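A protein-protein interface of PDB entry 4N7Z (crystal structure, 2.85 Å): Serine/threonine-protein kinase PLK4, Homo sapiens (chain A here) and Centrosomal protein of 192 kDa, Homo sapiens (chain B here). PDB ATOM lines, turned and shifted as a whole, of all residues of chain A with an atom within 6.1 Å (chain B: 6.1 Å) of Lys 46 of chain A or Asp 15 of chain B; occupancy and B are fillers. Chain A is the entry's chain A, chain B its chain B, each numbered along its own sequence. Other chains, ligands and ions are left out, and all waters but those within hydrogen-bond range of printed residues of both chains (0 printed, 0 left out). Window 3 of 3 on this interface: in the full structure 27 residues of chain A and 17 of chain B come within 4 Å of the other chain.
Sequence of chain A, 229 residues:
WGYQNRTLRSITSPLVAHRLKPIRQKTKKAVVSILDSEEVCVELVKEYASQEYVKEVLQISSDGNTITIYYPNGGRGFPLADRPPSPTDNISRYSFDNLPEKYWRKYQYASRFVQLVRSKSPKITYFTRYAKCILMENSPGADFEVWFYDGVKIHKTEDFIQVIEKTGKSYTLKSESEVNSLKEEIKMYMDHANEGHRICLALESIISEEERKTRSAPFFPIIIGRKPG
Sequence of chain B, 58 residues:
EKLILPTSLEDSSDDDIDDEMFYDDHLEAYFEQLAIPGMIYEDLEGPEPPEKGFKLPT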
ATOM      1  N   LYS A  29     -33.104 -12.988   7.819  1.00  0.00           N
ATOM      2  CA  LYS A  29     -32.106 -13.086   6.770  1.00  0.00           C
ATOM      3  C   LYS A  29     -32.588 -12.757   5.370  1.00  0.00           C
ATOM      4  O   LYS A  29     -31.856 -12.782   4.432  1.00  0.00           O
ATOM      5  CB  LYS A  29     -31.453 -14.467   6.760  1.00  0.00           C
ATOM      6  CG  LYS A  29     -31.786 -15.375   7.922  1.00  0.00           C
ATOM      7  CD  LYS A  29     -30.533 -15.959   8.567  1.00  0.00           C
ATOM      8  CE  LYS A  29     -30.746 -16.330  10.043  1.00  0.00           C
ATOM      9  NZ  LYS A  29     -30.072 -17.585  10.503  1.00  0.00           N
ATOM     10  N   LEU A  44     -32.148 -11.588  -0.589  1.00  0.00           N
ATOM     11  CA  LEU A  44     -31.252 -12.116   0.448  1.00  0.00           C
ATOM     12  C   LEU A  44     -30.551 -10.976   1.221  1.00  0.00           C
ATOM     13  O   LEU A  44     -29.828 -10.164   0.632  1.00  0.00           O
ATOM     14  CB  LEU A  44     -30.222 -13.056  -0.176  1.00  0.00           C
ATOM     15  CG  LEU A  44     -29.983 -14.376   0.553  1.00  0.00           C
ATOM     16  CD1 LEU A  44     -31.285 -15.159   0.683  1.00  0.00           C
ATOM     17  CD2 LEU A  44     -28.899 -15.198  -0.156  1.00  0.00           C
ATOM     18  N   VAL A  45     -30.758 -10.925   2.538  1.00  0.00           N
ATOM     19  CA  VAL A  45     -30.324  -9.784   3.354  1.00  0.00           C
ATOM     20  C   VAL A  45     -29.218 -10.092   4.371  1.00  0.00           C
ATOM     21  O   VAL A  45     -29.389 -10.949   5.229  1.00  0.00           O
ATOM     22  CB  VAL A  45     -31.517  -9.210   4.125  1.00  0.00           C
ATOM     23  CG1 VAL A  45     -31.076  -8.056   5.015  1.00  0.00           C
ATOM     24  CG2 VAL A  45     -32.612  -8.767   3.158  1.00  0.00           C
ATOM     25  N   LYS A  46     -28.124  -9.336   4.313  1.00  0.00           N
ATOM     26  CA  LYS A  46     -27.050  -9.459   5.298  1.00  0.00           C
ATOM     27  C   LYS A  46     -26.729  -8.115   5.962  1.00  0.00           C
ATOM     28  O   LYS A  46     -26.722  -7.076   5.302  1.00  0.00           O
ATOM     29  CB  LYS A  46     -25.791 -10.039   4.650  1.00  0.00           C
ATOM     30  CG  LYS A  46     -25.148 -11.166   5.442  1.00  0.00           C
ATOM     31  CD  LYS A  46     -26.038 -12.397   5.474  1.00  0.00           C
ATOM     32  CE  LYS A  46     -25.777 -13.236   6.714  1.00  0.00           C
ATOM     33  NZ  LYS A  46     -25.741 -14.692   6.402  1.00  0.00           N
ATOM     34  N   GLU A  47     -26.461  -8.142   7.267  1.00  0.00           N
ATOM     35  CA  GLU A  47     -26.117  -6.926   8.015  1.00  0.00           C
ATOM     36  C   GLU A  47     -24.600  -6.744   8.102  1.00  0.00           C
ATOM     37  O   GLU A  47     -23.871  -7.722   8.279  1.00  0.00           O
ATOM     38  CB  GLU A  47     -26.727  -6.975   9.426  1.00  0.00           C
ATOM     39  CG  GLU A  47     -26.434  -5.752  10.305  1.00  0.00           C
ATOM     40  CD  GLU A  47     -25.787  -6.123  11.626  1.00  0.00           C
ATOM     41  OE1 GLU A  47     -25.103  -7.171  11.676  1.00  0.00           O
ATOM     42  OE2 GLU A  47     -25.959  -5.368  12.607  1.00  0.00           O
ATOM     43  N   TYR A  48     -24.137  -5.538   7.871  1.00  0.00           N
ATOM     44  CA  TYR A  48     -22.769  -5.150   8.093  1.00  0.00           C
ATOM     45  C   TYR A  48     -22.775  -3.754   8.680  1.00  0.00           C
ATOM     46  O   TYR A  48     -23.525  -2.937   8.220  1.00  0.00           O
ATOM     47  CB  TYR A  48     -22.005  -5.176   6.773  1.00  0.00           C
ATOM     48  CG  TYR A  48     -20.679  -4.476   6.821  1.00  0.00           C
ATOM     49  CD1 TYR A  48     -19.553  -5.101   7.286  1.00  0.00           C
ATOM     50  CD2 TYR A  48     -20.567  -3.186   6.420  1.00  0.00           C
ATOM     51  CE1 TYR A  48     -18.360  -4.435   7.347  1.00  0.00           C
ATOM     52  CE2 TYR A  48     -19.381  -2.536   6.475  1.00  0.00           C
ATOM     53  CZ  TYR A  48     -18.294  -3.169   6.942  1.00  0.00           C
ATOM     54  OH  TYR A  48     -17.154  -2.489   6.950  1.00  0.00           O
ATOM     55  N   GLN A  51     -25.896  -1.668   9.661  1.00  0.00           N
ATOM     56  CA  GLN A  51     -26.988  -1.537   8.688  1.00  0.00           C
ATOM     57  C   GLN A  51     -27.207  -2.826   7.869  1.00  0.00           C
ATOM     58  O   GLN A  51     -26.322  -3.684   7.807  1.00  0.00           O
ATOM     59  CB  GLN A  51     -26.796  -0.315   7.781  1.00  0.00           C
ATOM     60  CG  GLN A  51     -28.019   0.625   7.749  1.00  0.00           C
ATOM     61  CD  GLN A  51     -28.557   0.982   9.152  1.00  0.00           C
ATOM     62  OE1 GLN A  51     -29.416   0.277   9.706  1.00  0.00           O
ATOM     63  NE2 GLN A  51     -28.055   2.085   9.721  1.00  0.00           N
ATOM     64  N   GLU A  52     -28.393  -2.958   7.265  1.00  0.00           N
ATOM     65  CA  GLU A  52     -28.774  -4.149   6.495  1.00  0.00           C
ATOM     66  C   GLU A  52     -28.616  -3.910   4.988  1.00  0.00           C
ATOM     67  O   GLU A  52     -28.996  -2.840   4.491  1.00  0.00           O
ATOM     68  CB  GLU A  52     -30.230  -4.534   6.813  1.00  0.00           C
ATOM     69  CG  GLU A  52     -30.407  -5.494   7.991  1.00  0.00           C
ATOM     70  CD  GLU A  52     -31.854  -5.629   8.431  1.00  0.00           C
ATOM     71  OE1 GLU A  52     -32.174  -6.606   9.147  1.00  0.00           O
ATOM     72  OE2 GLU A  52     -32.668  -4.752   8.069  1.00  0.00           O
ATOM     73  N   TYR A  53     -28.072  -4.893   4.261  1.00  0.00           N
ATOM     74  CA  TYR A  53     -27.920  -4.786   2.796  1.00  0.00           C
ATOM     75  C   TYR A  53     -28.611  -5.933   2.028  1.00  0.00           C
ATOM     76  O   TYR A  53     -29.212  -6.812   2.640  1.00  0.00           O
ATOM     77  CB  TYR A  53     -26.439  -4.723   2.404  1.00  0.00           C
ATOM     78  CG  TYR A  53     -25.666  -3.544   2.966  1.00  0.00           C
ATOM     79  CD1 TYR A  53     -25.255  -3.525   4.291  1.00  0.00           C
ATOM     80  CD2 TYR A  53     -25.325  -2.467   2.162  1.00  0.00           C
ATOM     81  CE1 TYR A  53     -24.546  -2.456   4.802  1.00  0.00           C
ATOM     82  CE2 TYR A  53     -24.606  -1.395   2.662  1.00  0.00           C
ATOM     83  CZ  TYR A  53     -24.220  -1.394   3.984  1.00  0.00           C
ATOM     84  OH  TYR A  53     -23.501  -0.330   4.493  1.00  0.00           O
ATOM     85  N   VAL A  54     -28.520  -5.925   0.697  1.00  0.00           N
ATOM     86  CA  VAL A  54     -29.103  -6.996  -0.134  1.00  0.00           C
ATOM     87  C   VAL A  54     -28.057  -7.683  -1.028  1.00  0.00           C
ATOM     88  O   VAL A  54     -27.572  -7.085  -1.988  1.00  0.00           O
ATOM     89  CB  VAL A  54     -30.275  -6.465  -1.005  1.00  0.00           C
ATOM     90  CG1 VAL A  54     -30.763  -7.529  -1.964  1.00  0.00           C
ATOM     91  CG2 VAL A  54     -31.422  -5.997  -0.128  1.00  0.00           C
ATOM     92  N   LYS A  55     -27.711  -8.933  -0.715  1.00  0.00           N
ATOM     93  CA  LYS A  55     -26.658  -9.630  -1.457  1.00  0.00           C
ATOM     94  C   LYS A  55     -27.092 -10.134  -2.826  1.00  0.00           C
ATOM     95  O   LYS A  55     -26.448  -9.829  -3.830  1.00  0.00           O
ATOM     96  CB  LYS A  55     -26.055 -10.778  -0.650  1.00  0.00           C
ATOM     97  CG  LYS A  55     -24.870 -11.433  -1.364  1.00  0.00           C
ATOM     98  CD  LYS A  55     -23.935 -12.109  -0.387  1.00  0.00           C
ATOM     99  CE  LYS A  55     -24.674 -13.139   0.440  1.00  0.00           C
ATOM    100  NZ  LYS A  55     -23.758 -13.763   1.425  1.00  0.00           N
ATOM    101  N   ASP B  14     -23.223 -16.637   2.633  1.00  0.00           N
ATOM    102  CA  ASP B  14     -24.556 -17.123   2.373  1.00  0.00           C
ATOM    103  C   ASP B  14     -24.866 -18.277   3.285  1.00  0.00           C
ATOM    104  O   ASP B  14     -24.777 -19.433   2.870  1.00  0.00           O
ATOM    105  CB  ASP B  14     -24.662 -17.564   0.924  1.00  0.00           C
ATOM    106  CG  ASP B  14     -26.013 -18.121   0.565  1.00  0.00           C
ATOM    107  OD1 ASP B  14     -26.784 -18.553   1.419  1.00  0.00           O
ATOM    108  OD2 ASP B  14     -26.310 -18.129  -0.625  1.00  0.00           O
ATOM    109  N   ASP B  15     -25.266 -17.983   4.511  1.00  0.00           N
ATOM    110  CA  ASP B  15     -25.954 -18.981   5.284  1.00  0.00           C
ATOM    111  C   ASP B  15     -27.377 -18.954   4.789  1.00  0.00           C
ATOM    112  O   ASP B  15     -27.805 -17.993   4.176  1.00  0.00           O
ATOM    113  CB  ASP B  15     -25.753 -18.859   6.793  1.00  0.00           C
ATOM    114  CG  ASP B  15     -26.820 -18.112   7.453  1.00  0.00           C
ATOM    115  OD1 ASP B  15     -27.174 -17.061   6.919  1.00  0.00           O
ATOM    116  OD2 ASP B  15     -27.330 -18.581   8.471  1.00  0.00           O
ATOM    117  N   ASP B  16     -27.982 -20.130   4.942  1.00  0.00           N
ATOM    118  CA  ASP B  16     -29.204 -20.563   4.289  1.00  0.00           C
ATOM    119  C   ASP B  16     -30.426 -19.910   4.874  1.00  0.00           C
ATOM    120  O   ASP B  16     -30.402 -19.411   6.000  1.00  0.00           O
ATOM    121  CB  ASP B  16     -29.339 -22.086   4.369  1.00  0.00           C
ATOM    122  CG  ASP B  16     -28.000 -22.794   4.293  1.00  0.00           C
ATOM    123  OD1 ASP B  16     -27.858 -23.869   4.912  1.00  0.00           O
ATOM    124  OD2 ASP B  16     -27.089 -22.275   3.613  1.00  0.00           O
ATOM    125  N   ILE B  17     -31.502 -19.905   4.102  1.00  0.00           N
ATOM    126  CA  ILE B  17     -32.669 -19.215   4.540  1.00  0.00           C
ATOM    127  C   ILE B  17     -33.752 -20.164   4.904  1.00  0.00           C
ATOM    128  O   ILE B  17     -34.766 -19.765   5.401  1.00  0.00           O
ATOM    129  CB  ILE B  17     -33.244 -18.397   3.395  1.00  0.00           C
ATOM    130  CG1 ILE B  17     -34.410 -17.523   3.844  1.00  0.00           C
ATOM    131  CG2 ILE B  17     -33.711 -19.311   2.302  1.00  0.00           C
ATOM    132  CD1 ILE B  17     -34.841 -16.461   2.861  1.00  0.00           C
ATOM    133  N   ASP B  19     -34.405 -21.786   7.110  1.00  0.00           N
ATOM    134  CA  ASP B  19     -34.865 -21.595   8.434  1.00  0.00           C
ATOM    135  C   ASP B  19     -36.039 -20.636   8.498  1.00  0.00           C
ATOM    136  O   ASP B  19     -36.998 -20.909   9.187  1.00  0.00           O
ATOM    137  CB  ASP B  19     -33.698 -21.063   9.261  1.00  0.00           C
ATOM    138  CG  ASP B  19     -32.404 -21.770   8.956  1.00  0.00           C
ATOM    139  OD1 ASP B  19     -31.487 -21.160   8.382  1.00  0.00           O
ATOM    140  OD2 ASP B  19     -32.316 -22.954   9.269  1.00  0.00           O
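The side-chain amino group (NZ) of Lys 46 of chain A lies within salt-bridge range of the side-chain carboxylate (OD1) of Asp 15 of chain B, 2.8 Å away.
NZ of Lys 29 of chain A lies within salt-bridge range of OD2 of Asp 15 of chain B, 3.6 Å away.
The backbone NH (N) of Asp 14 of chain B sits close to the side-chain amino group (NZ) of Lys 55 of chain A.
O of Leu 44 of chain A lies within hydrogen-bond range of N of Lys 55 of chain A, at 2.8 Å.
The backbone carbonyl oxygen (O) of Lys 29 of chain A sits at hydrogen-bond distance from the backbone NH (N) of Val 45 of chain A.
The backbone carbonyl oxygen (O) of Lys 46 of chain A sits at hydrogen-bond distance from the backbone NH (N) of Tyr 53 of chain A, at 2.8 Å.
Among the printed residues, merely in contact across the chains: Leu 44 of chain A with Asp 14 of chain B.
Asp 15 of chain B touches just these residues of chain A: Lys 29 (3.6 Å) and Lys 46 (2.8 Å).
Of the printed residues of chain B, Leu 44 of chain A touches Asp 14.
Of the printed residues of chain A, Asp 14 of chain B touches Leu 44 and Lys 55.
Of the printed residues of chain B, Lys 55 of chain A touches Asp 14.
The nearest residue of chain B that does not touch Lys 46 of chain A is Asp 14 of chain B (4.8 Å).
The nearest residue of chain A that does not touch Asp 15 of chain B is Leu 44 of chain A (5.3 Å).
Of the 11 printed residues of chain A, 4 touch a printed residue of chain B.
Printed residues of chain B that touch a printed residue of chain A: Asp 14 and Asp 15.
Among the printed residues, Asp or Glu carboxylates within 4 Å of a Lys or Arg side-chain nitrogen of the other chain: Lys 29 of chain A with Asp 15 of chain B (3.6 Å) and Lys 46 of chain A with Asp 15 of chain B (2.8 Å).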
